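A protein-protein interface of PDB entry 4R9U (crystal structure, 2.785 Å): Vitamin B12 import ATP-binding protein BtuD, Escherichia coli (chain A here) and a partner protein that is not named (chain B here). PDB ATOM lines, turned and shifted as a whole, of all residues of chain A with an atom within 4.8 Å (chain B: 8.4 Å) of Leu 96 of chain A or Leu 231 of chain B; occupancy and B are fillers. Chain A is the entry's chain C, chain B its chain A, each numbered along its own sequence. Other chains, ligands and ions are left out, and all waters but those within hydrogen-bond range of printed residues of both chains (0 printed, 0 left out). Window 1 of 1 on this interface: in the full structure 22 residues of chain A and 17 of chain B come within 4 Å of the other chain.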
ATOM      1  N   ALA A  72      -6.982 -20.980  12.342  1.00  0.00           N
ATOM      2  CA  ALA A  72      -7.455 -22.217  11.733  1.00  0.00           C
ATOM      3  C   ALA A  72      -6.319 -23.167  11.372  1.00  0.00           C
ATOM      4  O   ALA A  72      -6.539 -24.177  10.708  1.00  0.00           O
ATOM      5  CB  ALA A  72      -8.289 -21.912  10.491  1.00  0.00           C
ATOM      6  N   HIS A  92     -14.818 -33.133  -2.011  1.00  0.00           N
ATOM      7  CA  HIS A  92     -14.598 -31.705  -2.156  1.00  0.00           C
ATOM      8  C   HIS A  92     -14.689 -31.063  -0.791  1.00  0.00           C
ATOM      9  O   HIS A  92     -13.893 -30.204  -0.440  1.00  0.00           O
ATOM     10  CB  HIS A  92     -15.616 -31.088  -3.123  1.00  0.00           C
ATOM     11  CG  HIS A  92     -15.447 -29.613  -3.321  1.00  0.00           C
ATOM     12  ND1 HIS A  92     -16.516 -28.753  -3.483  1.00  0.00           N
ATOM     13  CD2 HIS A  92     -14.332 -28.845  -3.366  1.00  0.00           C
ATOM     14  CE1 HIS A  92     -16.064 -27.520  -3.625  1.00  0.00           C
ATOM     15  NE2 HIS A  92     -14.743 -27.549  -3.557  1.00  0.00           N
ATOM     16  N   TYR A  93     -15.710 -31.453  -0.036  1.00  0.00           N
ATOM     17  CA  TYR A  93     -15.869 -30.905   1.298  1.00  0.00           C
ATOM     18  C   TYR A  93     -14.639 -31.198   2.132  1.00  0.00           C
ATOM     19  O   TYR A  93     -14.133 -30.340   2.846  1.00  0.00           O
ATOM     20  CB  TYR A  93     -17.096 -31.483   1.983  1.00  0.00           C
ATOM     21  CG  TYR A  93     -17.338 -30.959   3.381  1.00  0.00           C
ATOM     22  CD1 TYR A  93     -18.073 -29.808   3.558  1.00  0.00           C
ATOM     23  CD2 TYR A  93     -16.843 -31.592   4.513  1.00  0.00           C
ATOM     24  CE1 TYR A  93     -18.342 -29.304   4.803  1.00  0.00           C
ATOM     25  CE2 TYR A  93     -17.106 -31.081   5.800  1.00  0.00           C
ATOM     26  CZ  TYR A  93     -17.862 -29.930   5.925  1.00  0.00           C
ATOM     27  OH  TYR A  93     -18.165 -29.366   7.146  1.00  0.00           O
ATOM     28  N   LEU A  94     -14.148 -32.418   2.010  1.00  0.00           N
ATOM     29  CA  LEU A  94     -12.996 -32.829   2.782  1.00  0.00           C
ATOM     30  C   LEU A  94     -11.766 -32.036   2.322  1.00  0.00           C
ATOM     31  O   LEU A  94     -11.171 -31.298   3.118  1.00  0.00           O
ATOM     32  CB  LEU A  94     -12.753 -34.330   2.644  1.00  0.00           C
ATOM     33  CG  LEU A  94     -13.730 -35.267   3.362  1.00  0.00           C
ATOM     34  CD1 LEU A  94     -13.496 -36.717   2.936  1.00  0.00           C
ATOM     35  CD2 LEU A  94     -13.589 -35.144   4.856  1.00  0.00           C
ATOM     36  N   THR A  95     -11.412 -32.145   1.043  1.00  0.00           N
ATOM     37  CA  THR A  95     -10.223 -31.456   0.538  1.00  0.00           C
ATOM     38  C   THR A  95     -10.232 -29.939   0.750  1.00  0.00           C
ATOM     39  O   THR A  95      -9.208 -29.283   0.620  1.00  0.00           O
ATOM     40  CB  THR A  95      -9.976 -31.744  -0.973  1.00  0.00           C
ATOM     41  OG1 THR A  95     -11.158 -31.452  -1.715  1.00  0.00           O
ATOM     42  CG2 THR A  95      -9.649 -33.204  -1.193  1.00  0.00           C
ATOM     43  N   LEU A  96     -11.391 -29.405   1.130  1.00  0.00           N
ATOM     44  CA  LEU A  96     -11.517 -27.989   1.368  1.00  0.00           C
ATOM     45  C   LEU A  96     -10.985 -27.640   2.755  1.00  0.00           C
ATOM     46  O   LEU A  96     -10.696 -26.472   3.047  1.00  0.00           O
ATOM     47  CB  LEU A  96     -12.974 -27.604   1.249  1.00  0.00           C
ATOM     48  CG  LEU A  96     -13.320 -26.447   0.348  1.00  0.00           C
ATOM     49  CD1 LEU A  96     -14.810 -26.149   0.469  1.00  0.00           C
ATOM     50  CD2 LEU A  96     -12.492 -25.262   0.763  1.00  0.00           C
ATOM     51  N   HIS A  97     -10.762 -28.665   3.572  1.00  0.00           N
ATOM     52  CA  HIS A  97     -10.365 -28.429   4.945  1.00  0.00           C
ATOM     53  C   HIS A  97      -8.881 -28.664   5.084  1.00  0.00           C
ATOM     54  O   HIS A  97      -8.275 -28.251   6.073  1.00  0.00           O
ATOM     55  CB  HIS A  97     -11.095 -29.349   5.916  1.00  0.00           C
ATOM     56  CG  HIS A  97     -12.475 -28.905   6.280  1.00  0.00           C
ATOM     57  ND1 HIS A  97     -13.574 -29.140   5.482  1.00  0.00           N
ATOM     58  CD2 HIS A  97     -12.935 -28.227   7.361  1.00  0.00           C
ATOM     59  CE1 HIS A  97     -14.656 -28.645   6.062  1.00  0.00           C
ATOM     60  NE2 HIS A  97     -14.295 -28.077   7.200  1.00  0.00           N
ATOM     61  N   GLN A  98      -8.293 -29.306   4.082  1.00  0.00           N
ATOM     62  CA  GLN A  98      -6.870 -29.590   4.101  1.00  0.00           C
ATOM     63  C   GLN A  98      -6.073 -28.327   3.828  1.00  0.00           C
ATOM     64  O   GLN A  98      -6.426 -27.526   2.959  1.00  0.00           O
ATOM     65  CB  GLN A  98      -6.520 -30.653   3.075  1.00  0.00           C
ATOM     66  CG  GLN A  98      -6.738 -32.064   3.539  1.00  0.00           C
ATOM     67  CD  GLN A  98      -6.240 -33.075   2.529  1.00  0.00           C
ATOM     68  OE1 GLN A  98      -6.709 -33.118   1.386  1.00  0.00           O
ATOM     69  NE2 GLN A  98      -5.263 -33.877   2.932  1.00  0.00           N
ATOM     70  N   LYS A 101      -3.282 -29.675   0.230  1.00  0.00           N
ATOM     71  CA  LYS A 101      -4.058 -30.494  -0.702  1.00  0.00           C
ATOM     72  C   LYS A 101      -3.229 -31.585  -1.398  1.00  0.00           C
ATOM     73  O   LYS A 101      -3.778 -32.462  -2.060  1.00  0.00           O
ATOM     74  CB  LYS A 101      -4.710 -29.609  -1.765  1.00  0.00           C
ATOM     75  CG  LYS A 101      -4.950 -28.151  -1.352  1.00  0.00           C
ATOM     76  CD  LYS A 101      -6.257 -27.970  -0.572  1.00  0.00           C
ATOM     77  CE  LYS A 101      -6.590 -26.493  -0.357  1.00  0.00           C
ATOM     78  NZ  LYS A 101      -7.893 -26.291   0.338  1.00  0.00           N
ATOM     79  N   GLN A 143      -8.083 -31.183   8.986  1.00  0.00           N
ATOM     80  CA  GLN A 143      -7.617 -29.826   9.152  1.00  0.00           C
ATOM     81  C   GLN A 143      -6.558 -29.732  10.230  1.00  0.00           C
ATOM     82  O   GLN A 143      -5.693 -28.876  10.164  1.00  0.00           O
ATOM     83  CB  GLN A 143      -8.780 -28.876   9.444  1.00  0.00           C
ATOM     84  CG  GLN A 143      -8.365 -27.502   9.872  1.00  0.00           C
ATOM     85  CD  GLN A 143      -9.551 -26.689  10.266  1.00  0.00           C
ATOM     86  OE1 GLN A 143     -10.692 -27.064   9.978  1.00  0.00           O
ATOM     87  NE2 GLN A 143      -9.303 -25.526  10.861  1.00  0.00           N
ATOM     88  N   SER B 215     -11.715 -17.783  -5.748  1.00  0.00           N
ATOM     89  CA  SER B 215     -12.658 -18.884  -5.739  1.00  0.00           C
ATOM     90  C   SER B 215     -12.723 -19.518  -4.379  1.00  0.00           C
ATOM     91  O   SER B 215     -13.808 -19.811  -3.881  1.00  0.00           O
ATOM     92  CB  SER B 215     -12.261 -19.944  -6.776  1.00  0.00           C
ATOM     93  OG  SER B 215     -11.103 -19.575  -7.507  1.00  0.00           O
ATOM     94  N   ARG B 216     -11.559 -19.726  -3.777  1.00  0.00           N
ATOM     95  CA  ARG B 216     -11.478 -20.332  -2.452  1.00  0.00           C
ATOM     96  C   ARG B 216     -12.453 -19.736  -1.438  1.00  0.00           C
ATOM     97  O   ARG B 216     -13.301 -20.462  -0.907  1.00  0.00           O
ATOM     98  CB  ARG B 216     -10.060 -20.228  -1.912  1.00  0.00           C
ATOM     99  CG  ARG B 216      -9.809 -21.203  -0.807  1.00  0.00           C
ATOM    100  CD  ARG B 216      -8.519 -20.906  -0.091  1.00  0.00           C
ATOM    101  NE  ARG B 216      -8.659 -21.026   1.354  1.00  0.00           N
ATOM    102  CZ  ARG B 216      -8.782 -22.182   1.999  1.00  0.00           C
ATOM    103  NH1 ARG B 216      -8.891 -22.190   3.320  1.00  0.00           N
ATOM    104  NH2 ARG B 216      -8.806 -23.329   1.329  1.00  0.00           N
ATOM    105  N   PRO B 217     -12.361 -18.412  -1.174  1.00  0.00           N
ATOM    106  CA  PRO B 217     -13.240 -17.887  -0.122  1.00  0.00           C
ATOM    107  C   PRO B 217     -14.712 -18.032  -0.472  1.00  0.00           C
ATOM    108  O   PRO B 217     -15.549 -18.155   0.416  1.00  0.00           O
ATOM    109  CB  PRO B 217     -12.855 -16.416  -0.048  1.00  0.00           C
ATOM    110  CG  PRO B 217     -12.426 -16.103  -1.426  1.00  0.00           C
ATOM    111  CD  PRO B 217     -11.681 -17.320  -1.887  1.00  0.00           C
ATOM    112  N   MET B 218     -15.041 -18.023  -1.756  1.00  0.00           N
ATOM    113  CA  MET B 218     -16.438 -18.179  -2.127  1.00  0.00           C
ATOM    114  C   MET B 218     -16.855 -19.618  -1.942  1.00  0.00           C
ATOM    115  O   MET B 218     -18.006 -19.879  -1.575  1.00  0.00           O
ATOM    116  CB  MET B 218     -16.695 -17.713  -3.560  1.00  0.00           C
ATOM    117  CG  MET B 218     -16.235 -16.280  -3.837  1.00  0.00           C
ATOM    118  SD  MET B 218     -17.622 -15.189  -3.991  1.00  0.00           S
ATOM    119  CE  MET B 218     -18.492 -15.494  -2.451  1.00  0.00           C
ATOM    120  N   ASN B 219     -15.941 -20.556  -2.183  1.00  0.00           N
ATOM    121  CA  ASN B 219     -16.248 -21.948  -1.861  1.00  0.00           C
ATOM    122  C   ASN B 219     -16.442 -22.165  -0.397  1.00  0.00           C
ATOM    123  O   ASN B 219     -17.143 -23.082  -0.002  1.00  0.00           O
ATOM    124  CB  ASN B 219     -15.176 -22.909  -2.351  1.00  0.00           C
ATOM    125  CG  ASN B 219     -15.271 -23.179  -3.825  1.00  0.00           C
ATOM    126  OD1 ASN B 219     -16.359 -23.114  -4.396  1.00  0.00           O
ATOM    127  ND2 ASN B 219     -14.158 -23.534  -4.445  1.00  0.00           N
ATOM    128  N   MET B 220     -15.789 -21.346   0.411  1.00  0.00           N
ATOM    129  CA  MET B 220     -15.993 -21.440   1.845  1.00  0.00           C
ATOM    130  C   MET B 220     -17.315 -20.822   2.287  1.00  0.00           C
ATOM    131  O   MET B 220     -18.015 -21.390   3.115  1.00  0.00           O
ATOM    132  CB  MET B 220     -14.831 -20.795   2.581  1.00  0.00           C
ATOM    133  CG  MET B 220     -13.541 -21.549   2.383  1.00  0.00           C
ATOM    134  SD  MET B 220     -12.209 -20.743   3.275  1.00  0.00           S
ATOM    135  CE  MET B 220     -12.925 -20.690   4.896  1.00  0.00           C
ATOM    136  N   LEU B 221     -17.689 -19.694   1.683  1.00  0.00           N
ATOM    137  CA  LEU B 221     -18.957 -19.056   2.002  1.00  0.00           C
ATOM    138  C   LEU B 221     -20.112 -19.980   1.677  1.00  0.00           C
ATOM    139  O   LEU B 221     -21.187 -19.877   2.275  1.00  0.00           O
ATOM    140  CB  LEU B 221     -19.092 -17.740   1.232  1.00  0.00           C
ATOM    141  CG  LEU B 221     -18.557 -16.549   2.009  1.00  0.00           C
ATOM    142  CD1 LEU B 221     -18.317 -15.347   1.103  1.00  0.00           C
ATOM    143  CD2 LEU B 221     -19.577 -16.232   3.080  1.00  0.00           C
ATOM    144  N   ALA B 222     -19.870 -20.897   0.742  1.00  0.00           N
ATOM    145  CA  ALA B 222     -20.882 -21.835   0.277  1.00  0.00           C
ATOM    146  C   ALA B 222     -21.271 -22.790   1.413  1.00  0.00           C
ATOM    147  O   ALA B 222     -22.301 -23.455   1.342  1.00  0.00           O
ATOM    148  CB  ALA B 222     -20.393 -22.596  -0.965  1.00  0.00           C
ATOM    149  N   LEU B 223     -20.445 -22.875   2.460  1.00  0.00           N
ATOM    150  CA  LEU B 223     -20.848 -23.627   3.662  1.00  0.00           C
ATOM    151  C   LEU B 223     -21.439 -22.663   4.657  1.00  0.00           C
ATOM    152  O   LEU B 223     -21.806 -21.535   4.325  1.00  0.00           O
ATOM    153  CB  LEU B 223     -19.689 -24.349   4.332  1.00  0.00           C
ATOM    154  CG  LEU B 223     -18.513 -24.739   3.442  1.00  0.00           C
ATOM    155  CD1 LEU B 223     -17.251 -24.895   4.255  1.00  0.00           C
ATOM    156  CD2 LEU B 223     -18.818 -26.003   2.634  1.00  0.00           C
ATOM    157  N   GLY B 224     -21.447 -23.098   5.903  1.00  0.00           N
ATOM    158  CA  GLY B 224     -22.016 -22.296   6.961  1.00  0.00           C
ATOM    159  C   GLY B 224     -21.221 -21.024   7.115  1.00  0.00           C
ATOM    160  O   GLY B 224     -20.124 -20.893   6.584  1.00  0.00           O
ATOM    161  N   GLU B 225     -21.847 -20.035   7.724  1.00  0.00           N
ATOM    162  CA  GLU B 225     -21.139 -18.859   8.161  1.00  0.00           C
ATOM    163  C   GLU B 225     -19.995 -19.338   9.078  1.00  0.00           C
ATOM    164  O   GLU B 225     -18.809 -19.013   8.866  1.00  0.00           O
ATOM    165  CB  GLU B 225     -22.131 -17.942   8.877  1.00  0.00           C
ATOM    166  CG  GLU B 225     -21.909 -16.483   8.604  1.00  0.00           C
ATOM    167  CD  GLU B 225     -22.466 -15.559   9.670  1.00  0.00           C
ATOM    168  OE1 GLU B 225     -22.100 -15.723  10.863  1.00  0.00           O
ATOM    169  OE2 GLU B 225     -23.254 -14.652   9.295  1.00  0.00           O
ATOM    170  N   ILE B 226     -20.343 -20.221  10.015  1.00  0.00           N
ATOM    171  CA  ILE B 226     -19.436 -20.698  11.070  1.00  0.00           C
ATOM    172  C   ILE B 226     -18.352 -21.665  10.594  1.00  0.00           C
ATOM    173  O   ILE B 226     -17.199 -21.517  10.967  1.00  0.00           O
ATOM    174  CB  ILE B 226     -20.208 -21.399  12.211  1.00  0.00           C
ATOM    175  CG1 ILE B 226     -21.234 -20.426  12.800  1.00  0.00           C
ATOM    176  CG2 ILE B 226     -19.259 -21.880  13.296  1.00  0.00           C
ATOM    177  CD1 ILE B 226     -20.607 -19.371  13.642  1.00  0.00           C
ATOM    178  N   SER B 227     -18.724 -22.664   9.805  1.00  0.00           N
ATOM    179  CA  SER B 227     -17.737 -23.528   9.168  1.00  0.00           C
ATOM    180  C   SER B 227     -16.680 -22.715   8.417  1.00  0.00           C
ATOM    181  O   SER B 227     -15.494 -23.029   8.450  1.00  0.00           O
ATOM    182  CB  SER B 227     -18.391 -24.510   8.188  1.00  0.00           C
ATOM    183  OG  SER B 227     -19.785 -24.630   8.415  1.00  0.00           O
ATOM    184  N   ALA B 228     -17.132 -21.691   7.691  1.00  0.00           N
ATOM    185  CA  ALA B 228     -16.187 -20.846   6.985  1.00  0.00           C
ATOM    186  C   ALA B 228     -15.301 -20.053   7.958  1.00  0.00           C
ATOM    187  O   ALA B 228     -14.094 -20.013   7.784  1.00  0.00           O
ATOM    188  CB  ALA B 228     -16.914 -19.922   6.005  1.00  0.00           C
ATOM    189  N   ARG B 229     -15.880 -19.415   8.977  1.00  0.00           N
ATOM    190  CA  ARG B 229     -15.062 -18.663   9.949  1.00  0.00           C
ATOM    191  C   ARG B 229     -13.978 -19.586  10.539  1.00  0.00           C
ATOM    192  O   ARG B 229     -12.794 -19.234  10.648  1.00  0.00           O
ATOM    193  CB  ARG B 229     -15.955 -18.113  11.045  1.00  0.00           C
ATOM    194  CG  ARG B 229     -16.811 -16.953  10.560  1.00  0.00           C
ATOM    195  CD  ARG B 229     -17.585 -16.222  11.675  1.00  0.00           C
ATOM    196  NE  ARG B 229     -16.719 -15.725  12.736  1.00  0.00           N
ATOM    197  CZ  ARG B 229     -17.113 -15.554  13.991  1.00  0.00           C
ATOM    198  NH1 ARG B 229     -18.367 -15.832  14.326  1.00  0.00           N
ATOM    199  NH2 ARG B 229     -16.257 -15.101  14.904  1.00  0.00           N
ATOM    200  N   GLN B 230     -14.381 -20.803  10.846  1.00  0.00           N
ATOM    201  CA  GLN B 230     -13.515 -21.768  11.515  1.00  0.00           C
ATOM    202  C   GLN B 230     -12.406 -22.297  10.617  1.00  0.00           C
ATOM    203  O   GLN B 230     -11.264 -22.470  11.064  1.00  0.00           O
ATOM    204  CB  GLN B 230     -14.383 -22.923  12.034  1.00  0.00           C
ATOM    205  CG  GLN B 230     -13.650 -24.033  12.775  1.00  0.00           C
ATOM    206  CD  GLN B 230     -13.018 -25.090  11.856  1.00  0.00           C
ATOM    207  OE1 GLN B 230     -12.004 -25.698  12.208  1.00  0.00           O
ATOM    208  NE2 GLN B 230     -13.617 -25.313  10.681  1.00  0.00           N
ATOM    209  N   LEU B 231     -12.746 -22.558   9.363  1.00  0.00           N
ATOM    210  CA  LEU B 231     -11.783 -22.991   8.357  1.00  0.00           C
ATOM    211  C   LEU B 231     -10.745 -21.904   8.060  1.00  0.00           C
ATOM    212  O   LEU B 231      -9.777 -22.142   7.330  1.00  0.00           O
ATOM    213  CB  LEU B 231     -12.506 -23.393   7.074  1.00  0.00           C
ATOM    214  CG  LEU B 231     -12.344 -24.786   6.448  1.00  0.00           C
ATOM    215  CD1 LEU B 231     -12.730 -24.710   4.975  1.00  0.00           C
ATOM    216  CD2 LEU B 231     -10.936 -25.342   6.611  1.00  0.00           C
ATOM    217  N   GLY B 232     -10.965 -20.702   8.602  1.00  0.00           N
ATOM    218  CA  GLY B 232     -10.003 -19.625   8.472  1.00  0.00           C
ATOM    219  C   GLY B 232     -10.323 -18.479   7.534  1.00  0.00           C
ATOM    220  O   GLY B 232      -9.419 -17.899   6.938  1.00  0.00           O
ATOM    221  N   LEU B 233     -11.603 -18.150   7.402  1.00  0.00           N
ATOM    222  CA  LEU B 233     -12.015 -17.034   6.568  1.00  0.00           C
ATOM    223  C   LEU B 233     -12.356 -15.851   7.432  1.00  0.00           C
ATOM    224  O   LEU B 233     -13.008 -15.979   8.463  1.00  0.00           O
ATOM    225  CB  LEU B 233     -13.225 -17.381   5.719  1.00  0.00           C
ATOM    226  CG  LEU B 233     -13.563 -16.436   4.572  1.00  0.00           C
ATOM    227  CD1 LEU B 233     -12.522 -16.667   3.496  1.00  0.00           C
ATOM    228  CD2 LEU B 233     -14.974 -16.687   4.060  1.00  0.00           C
ATOM    229  N   PRO B 234     -11.927 -14.681   7.017  1.00  0.00           N
ATOM    230  CA  PRO B 234     -12.347 -13.493   7.744  1.00  0.00           C
ATOM    231  C   PRO B 234     -13.617 -12.919   7.133  1.00  0.00           C
ATOM    232  O   PRO B 234     -13.550 -12.119   6.201  1.00  0.00           O
ATOM    233  CB  PRO B 234     -11.173 -12.544   7.570  1.00  0.00           C
ATOM    234  CG  PRO B 234     -10.541 -12.964   6.272  1.00  0.00           C
ATOM    235  CD  PRO B 234     -10.861 -14.410   6.046  1.00  0.00           C
ATOM    236  N   ASP B 278     -19.019 -25.547  -8.160  1.00  0.00           N
ATOM    237  CA  ASP B 278     -17.716 -25.097  -7.726  1.00  0.00           C
ATOM    238  C   ASP B 278     -17.404 -23.711  -8.226  1.00  0.00           C
ATOM    239  O   ASP B 278     -17.644 -23.382  -9.383  1.00  0.00           O
ATOM    240  CB  ASP B 278     -16.631 -26.052  -8.200  1.00  0.00           C
ATOM    241  CG  ASP B 278     -15.373 -25.949  -7.367  1.00  0.00           C
ATOM    242  OD1 ASP B 278     -15.188 -24.908  -6.699  1.00  0.00           O
ATOM    243  OD2 ASP B 278     -14.554 -26.891  -7.394  1.00  0.00           O
ATOM    244  N   ARG B 280     -14.369 -22.321  -8.605  1.00  0.00           N
ATOM    245  CA  ARG B 280     -13.212 -22.274  -9.492  1.00  0.00           C
ATOM    246  C   ARG B 280     -13.637 -22.484 -10.957  1.00  0.00           C
ATOM    247  O   ARG B 280     -12.896 -22.146 -11.871  1.00  0.00           O
ATOM    248  CB  ARG B 280     -12.113 -23.244  -9.016  1.00  0.00           C
ATOM    249  CG  ARG B 280     -12.578 -24.573  -8.433  1.00  0.00           C
ATOM    250  CD  ARG B 280     -11.407 -25.362  -7.832  1.00  0.00           C
ATOM    251  NE  ARG B 280     -11.099 -24.755  -6.536  1.00  0.00           N
ATOM    252  CZ  ARG B 280     -11.157 -25.365  -5.349  1.00  0.00           C
ATOM    253  NH1 ARG B 280     -10.887 -24.671  -4.245  1.00  0.00           N
ATOM    254  NH2 ARG B 280     -11.461 -26.656  -5.250  1.00  0.00           N
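The side-chain amide oxygen (OE1) of Gln 143 of chain A lies close to the side-chain amide oxygen (OE1) of Gln 230 of chain B.
NH2 of Arg 216 of chain B lies close to NZ of Lys 101 of chain A (3.3 Å).
The backbone carbonyl oxygen (O) of Thr 95 of chain A lies within hydrogen-bond range of the side-chain amino group (NZ) of Lys 101 of chain A.
OD2 of Asp 278 of chain B is in salt-bridge range of NH2 of Arg 280 of chain B.
The side-chain amide nitrogen of Asn 219 of chain B lies close to the guanidinium group of Arg 280 of chain B, at 3.5 Å.
ND2 of Asn 219 of chain B lies within hydrogen-bond range of OD1 of Asp 278 of chain B, at 2.8 Å.
The backbone carbonyl oxygen (O) of His 92 of chain A sits at hydrogen-bond distance from the side-chain hydroxyl (OG1) of Thr 95 of chain A (3.3 Å).
NH1 of Arg 216 of chain B sits at hydrogen-bond distance from SD of Met 220 of chain B (3.6 Å).
O of Gln 230 of chain B touches CB of Ala 72 of chain A, at 3.1 Å.
Leu 231 of chain B touches Ala 72 of chain A.
CB of Ala 72 of chain A touches N of Gly 232 of chain B (3.5 Å).
OD2 of Asp 278 of chain B touches NE2 of His 92 of chain A (3.9 Å).
His 92 of chain A touches Arg 280 of chain B (NE2 to NH2, 3.8 Å).
CD2 of Leu 223 of chain B touches CE1 of Tyr 93 of chain A, at 3.98 Å.
Asn 219 of chain B touches Leu 96 of chain A (O to CD1, 3.9 Å).
Leu 96 of chain A touches Leu 231 of chain B.
His 97 of chain A touches Leu 231 of chain B.
Gln 143 of chain A touches Leu 231 of chain B (OE1 to CD2, 3.8 Å).
Printed residues of chain B within 4 Å of His 92 of chain A: Asp 278 (3.9 Å) and Arg 280 (3.8 Å).
Of chain B, only Asn 219 and Leu 231 come within 4 Å of Leu 96 of chain A.
Of the printed residues of chain A, Asn 219 of chain B touches Leu 96 (3.9 Å).
Ala 228 of chain B touches none of the printed residues of chain A.
Of the printed residues of chain A, Gln 230 of chain B touches Ala 72 (3.1 Å) and Gln 143 (2.9 Å).
Pro 234 of chain B touches none of the printed residues of chain A.
The nearest residue of chain B that does not touch Leu 96 of chain A is Arg 216 of chain B (4.05 Å).
The nearest printed residue of chain A that does not touch Leu 231 of chain B is Gln 98 of chain A (5.4 Å).
Hydrophobic or aromatic side chains of chain B within 4 Å of the printed part of chain A: Leu 223 and Leu 231.
Hydrophobic or aromatic side chains of chain A that line the printed part of chain B: Ala 72, His 92, Tyr 93, Leu 96 and His 97.
Among the printed residues, no Asp or Glu carboxylate lies within 4 Å of a Lys or Arg side-chain nitrogen of the other chain.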
